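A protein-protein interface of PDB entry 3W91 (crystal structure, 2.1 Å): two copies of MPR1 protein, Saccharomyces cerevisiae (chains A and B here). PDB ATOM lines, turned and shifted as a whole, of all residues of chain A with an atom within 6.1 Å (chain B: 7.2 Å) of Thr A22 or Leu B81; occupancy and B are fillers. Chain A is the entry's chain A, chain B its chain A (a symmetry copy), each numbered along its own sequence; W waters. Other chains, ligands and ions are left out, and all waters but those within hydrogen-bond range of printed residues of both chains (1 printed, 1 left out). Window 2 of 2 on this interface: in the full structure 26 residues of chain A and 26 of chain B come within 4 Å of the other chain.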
ATOM      1  N   GLY A  20      -0.981  -0.151 -11.067  1.00  0.00           N
ATOM      2  CA  GLY A  20      -1.510   0.566 -12.205  1.00  0.00           C
ATOM      3  C   GLY A  20      -2.812  -0.011 -12.774  1.00  0.00           C
ATOM      4  O   GLY A  20      -3.515  -0.772 -12.098  1.00  0.00           O
ATOM      5  N   PRO A  21      -3.167   0.410 -14.003  1.00  0.00           N
ATOM      6  CA  PRO A  21      -4.390  -0.048 -14.677  1.00  0.00           C
ATOM      7  C   PRO A  21      -4.359  -1.554 -14.905  1.00  0.00           C
ATOM      8  O   PRO A  21      -3.294  -2.122 -15.149  1.00  0.00           O
ATOM      9  CB  PRO A  21      -4.388   0.687 -16.031  1.00  0.00           C
ATOM     10  CG  PRO A  21      -3.128   1.476 -16.094  1.00  0.00           C
ATOM     11  CD  PRO A  21      -2.376   1.365 -14.797  1.00  0.00           C
ATOM     12  N   THR A  22      -5.519  -2.188 -14.834  1.00  0.00           N
ATOM     13  CA  THR A  22      -5.601  -3.625 -14.987  1.00  0.00           C
ATOM     14  C   THR A  22      -5.679  -4.058 -16.433  1.00  0.00           C
ATOM     15  O   THR A  22      -5.088  -5.068 -16.799  1.00  0.00           O
ATOM     16  CB  THR A  22      -6.824  -4.169 -14.243  1.00  0.00           C
ATOM     17  OG1 THR A  22      -6.673  -3.857 -12.853  1.00  0.00           O
ATOM     18  CG2 THR A  22      -6.957  -5.683 -14.427  1.00  0.00           C
ATOM     19  N   PHE A  23      -6.409  -3.304 -17.257  1.00  0.00           N
ATOM     20  CA  PHE A  23      -6.712  -3.778 -18.610  1.00  0.00           C
ATOM     21  C   PHE A  23      -5.829  -3.170 -19.699  1.00  0.00           C
ATOM     22  O   PHE A  23      -5.915  -3.562 -20.860  1.00  0.00           O
ATOM     23  CB  PHE A  23      -8.169  -3.489 -18.969  1.00  0.00           C
ATOM     24  CG  PHE A  23      -9.156  -4.355 -18.239  1.00  0.00           C
ATOM     25  CD1 PHE A  23      -9.633  -3.979 -16.992  1.00  0.00           C
ATOM     26  CD2 PHE A  23      -9.607  -5.538 -18.801  1.00  0.00           C
ATOM     27  CE1 PHE A  23     -10.542  -4.780 -16.313  1.00  0.00           C
ATOM     28  CE2 PHE A  23     -10.517  -6.343 -18.130  1.00  0.00           C
ATOM     29  CZ  PHE A  23     -10.985  -5.956 -16.883  1.00  0.00           C
ATOM     30  N   PHE A  24      -5.035  -2.167 -19.365  1.00  0.00           N
ATOM     31  CA  PHE A  24      -4.246  -1.535 -20.413  1.00  0.00           C
ATOM     32  C   PHE A  24      -2.777  -1.455 -20.030  1.00  0.00           C
ATOM     33  O   PHE A  24      -2.453  -1.080 -18.907  1.00  0.00           O
ATOM     34  CB  PHE A  24      -4.798  -0.138 -20.723  1.00  0.00           C
ATOM     35  CG  PHE A  24      -6.200  -0.153 -21.256  1.00  0.00           C
ATOM     36  CD1 PHE A  24      -6.436  -0.307 -22.619  1.00  0.00           C
ATOM     37  CD2 PHE A  24      -7.280  -0.042 -20.400  1.00  0.00           C
ATOM     38  CE1 PHE A  24      -7.727  -0.325 -23.114  1.00  0.00           C
ATOM     39  CE2 PHE A  24      -8.574  -0.080 -20.884  1.00  0.00           C
ATOM     40  CZ  PHE A  24      -8.799  -0.211 -22.246  1.00  0.00           C
ATOM     41  N   GLN A  25      -1.902  -1.782 -20.977  1.00  0.00           N
ATOM     42  CA  GLN A  25      -0.456  -1.719 -20.768  1.00  0.00           C
ATOM     43  C   GLN A  25       0.120  -0.325 -21.009  1.00  0.00           C
ATOM     44  O   GLN A  25      -0.497   0.517 -21.657  1.00  0.00           O
ATOM     45  CB  GLN A  25       0.260  -2.712 -21.696  1.00  0.00           C
ATOM     46  CG  GLN A  25       0.277  -4.138 -21.181  1.00  0.00           C
ATOM     47  CD  GLN A  25       1.118  -4.315 -19.920  1.00  0.00           C
ATOM     48  OE1 GLN A  25       2.349  -4.434 -19.984  1.00  0.00           O
ATOM     49  NE2 GLN A  25       0.451  -4.351 -18.763  1.00  0.00           N
ATOM     50  N   ALA A 130     -11.624   0.895  -8.885  1.00  0.00           N
ATOM     51  CA  ALA A 130     -11.325  -0.525  -8.959  1.00  0.00           C
ATOM     52  C   ALA A 130     -11.183  -0.990 -10.419  1.00  0.00           C
ATOM     53  O   ALA A 130     -11.517  -0.241 -11.346  1.00  0.00           O
ATOM     54  CB  ALA A 130     -12.398  -1.325  -8.200  1.00  0.00           C
ATOM     55  N   PRO A 131     -10.690  -2.228 -10.630  1.00  0.00           N
ATOM     56  CA  PRO A 131     -10.096  -2.643 -11.911  1.00  0.00           C
ATOM     57  C   PRO A 131     -10.864  -2.424 -13.234  1.00  0.00           C
ATOM     58  O   PRO A 131     -10.251  -1.997 -14.203  1.00  0.00           O
ATOM     59  CB  PRO A 131      -9.716  -4.108 -11.668  1.00  0.00           C
ATOM     60  CG  PRO A 131      -9.371  -4.111 -10.191  1.00  0.00           C
ATOM     61  CD  PRO A 131     -10.455  -3.238  -9.579  1.00  0.00           C
ATOM     62  N   ARG A 132     -12.157  -2.725 -13.306  1.00  0.00           N
ATOM     63  CA  ARG A 132     -12.876  -2.501 -14.572  1.00  0.00           C
ATOM     64  C   ARG A 132     -12.900  -1.029 -15.003  1.00  0.00           C
ATOM     65  O   ARG A 132     -13.067  -0.732 -16.190  1.00  0.00           O
ATOM     66  CB  ARG A 132     -14.301  -3.082 -14.514  1.00  0.00           C
ATOM     67  CG  ARG A 132     -14.312  -4.595 -14.347  1.00  0.00           C
ATOM     68  CD  ARG A 132     -15.724  -5.149 -14.420  1.00  0.00           C
ATOM     69  NE  ARG A 132     -15.703  -6.609 -14.475  1.00  0.00           N
ATOM     70  CZ  ARG A 132     -15.486  -7.293 -15.599  1.00  0.00           C
ATOM     71  NH1 ARG A 132     -15.269  -6.637 -16.728  1.00  0.00           N
ATOM     72  NH2 ARG A 132     -15.492  -8.626 -15.598  1.00  0.00           N
ATOM     73  N   SER A 134     -10.239   1.076 -14.046  1.00  0.00           N
ATOM     74  CA  SER A 134      -8.894   1.500 -13.642  1.00  0.00           C
ATOM     75  C   SER A 134      -8.123   2.220 -14.742  1.00  0.00           C
ATOM     76  O   SER A 134      -7.029   2.714 -14.489  1.00  0.00           O
ATOM     77  CB  SER A 134      -8.085   0.304 -13.149  1.00  0.00           C
ATOM     78  OG  SER A 134      -7.995  -0.645 -14.194  1.00  0.00           O
ATOM     79  N   HIS A 135      -8.701   2.323 -15.940  1.00  0.00           N
ATOM     80  CA  HIS A 135      -8.096   3.154 -16.993  1.00  0.00           C
ATOM     81  C   HIS A 135      -8.336   4.625 -16.780  1.00  0.00           C
ATOM     82  O   HIS A 135      -7.789   5.469 -17.517  1.00  0.00           O
ATOM     83  CB  HIS A 135      -8.562   2.715 -18.387  1.00  0.00           C
ATOM     84  CG  HIS A 135     -10.024   2.970 -18.648  1.00  0.00           C
ATOM     85  ND1 HIS A 135     -10.974   2.019 -18.475  1.00  0.00           N
ATOM     86  CD2 HIS A 135     -10.687   4.112 -19.072  1.00  0.00           C
ATOM     87  CE1 HIS A 135     -12.179   2.524 -18.793  1.00  0.00           C
ATOM     88  NE2 HIS A 135     -12.007   3.804 -19.162  1.00  0.00           N
ATOM     89  N   ILE B  72     -20.289  -9.618  -9.019  1.00  0.00           N
ATOM     90  CA  ILE B  72     -18.945  -9.273  -9.479  1.00  0.00           C
ATOM     91  C   ILE B  72     -18.557 -10.171 -10.669  1.00  0.00           C
ATOM     92  O   ILE B  72     -18.047  -9.675 -11.687  1.00  0.00           O
ATOM     93  CB  ILE B  72     -17.903  -9.411  -8.352  1.00  0.00           C
ATOM     94  CG1 ILE B  72     -18.108  -8.318  -7.289  1.00  0.00           C
ATOM     95  CG2 ILE B  72     -16.480  -9.420  -8.913  1.00  0.00           C
ATOM     96  CD1 ILE B  72     -17.191  -8.488  -6.085  1.00  0.00           C
ATOM     97  N   GLU B  73     -18.825 -11.476 -10.550  1.00  0.00           N
ATOM     98  CA  GLU B  73     -18.426 -12.436 -11.580  1.00  0.00           C
ATOM     99  C   GLU B  73     -19.160 -12.171 -12.902  1.00  0.00           C
ATOM    100  O   GLU B  73     -18.592 -12.337 -13.958  1.00  0.00           O
ATOM    101  CB  GLU B  73     -18.653 -13.890 -11.126  1.00  0.00           C
ATOM    102  CG  GLU B  73     -17.679 -14.423 -10.076  1.00  0.00           C
ATOM    103  CD  GLU B  73     -16.219 -14.299 -10.493  1.00  0.00           C
ATOM    104  OE1 GLU B  73     -15.397 -13.781  -9.705  1.00  0.00           O
ATOM    105  OE2 GLU B  73     -15.881 -14.708 -11.618  1.00  0.00           O
ATOM    106  N   GLY B  75     -19.894  -9.254 -13.970  1.00  0.00           N
ATOM    107  CA  GLY B  75     -19.087  -8.161 -14.500  1.00  0.00           C
ATOM    108  C   GLY B  75     -19.803  -7.032 -15.218  1.00  0.00           C
ATOM    109  O   GLY B  75     -19.245  -6.447 -16.147  1.00  0.00           O
ATOM    110  N   TYR B  78     -20.557  -3.633 -11.068  1.00  0.00           N
ATOM    111  CA  TYR B  78     -19.527  -3.107 -10.150  1.00  0.00           C
ATOM    112  C   TYR B  78     -18.163  -3.034 -10.846  1.00  0.00           C
ATOM    113  O   TYR B  78     -17.917  -3.769 -11.803  1.00  0.00           O
ATOM    114  CB  TYR B  78     -19.443  -3.996  -8.906  1.00  0.00           C
ATOM    115  CG  TYR B  78     -20.550  -3.758  -7.901  1.00  0.00           C
ATOM    116  CD1 TYR B  78     -21.834  -4.292  -8.090  1.00  0.00           C
ATOM    117  CD2 TYR B  78     -20.323  -2.973  -6.765  1.00  0.00           C
ATOM    118  CE1 TYR B  78     -22.858  -4.060  -7.175  1.00  0.00           C
ATOM    119  CE2 TYR B  78     -21.339  -2.756  -5.836  1.00  0.00           C
ATOM    120  CZ  TYR B  78     -22.598  -3.288  -6.057  1.00  0.00           C
ATOM    121  OH  TYR B  78     -23.583  -3.052  -5.127  1.00  0.00           O
ATOM    122  N   PRO B  79     -17.273  -2.139 -10.382  1.00  0.00           N
ATOM    123  CA  PRO B  79     -15.951  -2.017 -11.010  1.00  0.00           C
ATOM    124  C   PRO B  79     -14.983  -3.118 -10.545  1.00  0.00           C
ATOM    125  O   PRO B  79     -13.969  -3.386 -11.200  1.00  0.00           O
ATOM    126  CB  PRO B  79     -15.479  -0.633 -10.545  1.00  0.00           C
ATOM    127  CG  PRO B  79     -16.123  -0.454  -9.191  1.00  0.00           C
ATOM    128  CD  PRO B  79     -17.487  -1.106  -9.343  1.00  0.00           C
ATOM    129  N   GLN B  80     -15.290  -3.761  -9.432  1.00  0.00           N
ATOM    130  CA  GLN B  80     -14.509  -4.928  -9.007  1.00  0.00           C
ATOM    131  C   GLN B  80     -14.372  -5.963 -10.098  1.00  0.00           C
ATOM    132  O   GLN B  80     -15.300  -6.185 -10.872  1.00  0.00           O
ATOM    133  CB  GLN B  80     -15.111  -5.575  -7.761  1.00  0.00           C
ATOM    134  CG  GLN B  80     -14.726  -4.853  -6.487  1.00  0.00           C
ATOM    135  CD  GLN B  80     -15.451  -3.541  -6.380  1.00  0.00           C
ATOM    136  OE1 GLN B  80     -14.932  -2.577  -5.804  1.00  0.00           O
ATOM    137  NE2 GLN B  80     -16.653  -3.473  -6.967  1.00  0.00           N
ATOM    138  N   LEU B  81     -13.203  -6.593 -10.170  1.00  0.00           N
ATOM    139  CA  LEU B  81     -12.974  -7.639 -11.162  1.00  0.00           C
ATOM    140  C   LEU B  81     -12.980  -9.013 -10.507  1.00  0.00           C
ATOM    141  O   LEU B  81     -13.476  -9.962 -11.072  1.00  0.00           O
ATOM    142  CB  LEU B  81     -11.654  -7.416 -11.912  1.00  0.00           C
ATOM    143  CG  LEU B  81     -11.189  -8.519 -12.863  1.00  0.00           C
ATOM    144  CD1 LEU B  81     -12.171  -8.698 -14.019  1.00  0.00           C
ATOM    145  CD2 LEU B  81      -9.771  -8.265 -13.381  1.00  0.00           C
ATOM    146  N   HIS B  82     -12.428  -9.094  -9.308  1.00  0.00           N
ATOM    147  CA  HIS B  82     -12.247 -10.369  -8.637  1.00  0.00           C
ATOM    148  C   HIS B  82     -13.212 -10.554  -7.495  1.00  0.00           C
ATOM    149  O   HIS B  82     -13.567  -9.609  -6.807  1.00  0.00           O
ATOM    150  CB  HIS B  82     -10.812 -10.491  -8.137  1.00  0.00           C
ATOM    151  CG  HIS B  82      -9.811 -10.676  -9.241  1.00  0.00           C
ATOM    152  ND1 HIS B  82      -8.818  -9.793  -9.478  1.00  0.00           N
ATOM    153  CD2 HIS B  82      -9.689 -11.674 -10.200  1.00  0.00           C
ATOM    154  CE1 HIS B  82      -8.094 -10.213 -10.528  1.00  0.00           C
ATOM    155  NE2 HIS B  82      -8.630 -11.360 -10.971  1.00  0.00           N
ATOM    156  N   SER B  83     -13.644 -11.786  -7.308  1.00  0.00           N
ATOM    157  CA  SER B  83     -14.450 -12.172  -6.167  1.00  0.00           C
ATOM    158  C   SER B  83     -13.702 -11.896  -4.879  1.00  0.00           C
ATOM    159  O   SER B  83     -12.465 -11.957  -4.855  1.00  0.00           O
ATOM    160  CB  SER B  83     -14.749 -13.672  -6.255  1.00  0.00           C
ATOM    161  OG  SER B  83     -15.714 -13.897  -7.266  1.00  0.00           O
ATOM    162  N   ILE B 204     -14.912  -1.126 -18.404  1.00  0.00           N
ATOM    163  CA  ILE B 204     -14.777  -2.306 -19.252  1.00  0.00           C
ATOM    164  C   ILE B 204     -15.656  -3.408 -18.662  1.00  0.00           C
ATOM    165  O   ILE B 204     -15.312  -4.011 -17.631  1.00  0.00           O
ATOM    166  CB  ILE B 204     -13.310  -2.788 -19.326  1.00  0.00           C
ATOM    167  CG1 ILE B 204     -12.383  -1.651 -19.779  1.00  0.00           C
ATOM    168  CG2 ILE B 204     -13.169  -3.950 -20.309  1.00  0.00           C
ATOM    169  CD1 ILE B 204     -12.753  -1.083 -21.132  1.00  0.00           C
HETATM  170  O   HOH W   1     -15.606  -9.719 -12.718  1.00  0.00           O
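No position is printed for both chains. Of the 11 pairs that touch across the chains among the printed residues, none has its exchanged pair printed and touching as well.
Of the 10 printed residues of chain B, 6 touch a printed residue of chain A. Hydrophobic or aromatic side chains of chain B within 4 Å of the printed part of chain A: Pro B79, Leu B81 and Ile B204. Printed residues of chain A that touch a printed residue of chain B: Thr A22, Ala A130, Pro A131 and Arg A132. Hydrophobic or aromatic side chains of chain A that line the printed part of chain B: Ala A130 and Pro A131. Among the printed residues, 11 pairs touch across the chains.
Among the printed residues, merely in contact across the chains: Pro A131 with Pro B79, Arg A132 with Gln B80, Arg A132 with Leu B81, Arg A132 with Tyr B78, Ala A130 with Gln B80, Arg A132 with Gly B75, Ala A130 with Pro B79, Pro A131 with Leu B81 and Thr A22 with Leu B81.
O of Ile B204 lies within hydrogen-bond range of NH1 of Arg A132 (2.8 Å). N of Arg A132 is in hydrogen-bond range of O of Pro B79 (2.9 Å).
Water W1 lies within hydrogen-bond range of the backbone carbonyl oxygen of Ile B72 (2.7 Å), the backbone carbonyl oxygen of Leu B81 (2.7 Å) and the guanidinium group of Arg A132 (3.1 Å).
Printed residues of chain B within 4 Å of Ala A130: Pro B79 and Gln B80. Of the printed residues of chain B, Arg A132 touches Gly B75, Tyr B78, Pro B79, Gln B80, Leu B81 and Ile B204. Ile B72 touches none of the printed residues of chain A. Printed residues of chain A within 4 Å of Tyr B78: Arg A132. Leu B81 touches just these residues of chain A: Thr A22, Pro A131 and Arg A132. The nearest printed residue of chain B that does not touch Pro A131 is Gln B80 (4.4 Å).
OG of Ser A134 lies within hydrogen-bond range of N of Thr A22, 3.0 Å away. The side-chain hydroxyl (OG) of Ser A134 lies within hydrogen-bond range of the backbone carbonyl oxygen (O) of Pro A131, at 2.6 Å.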
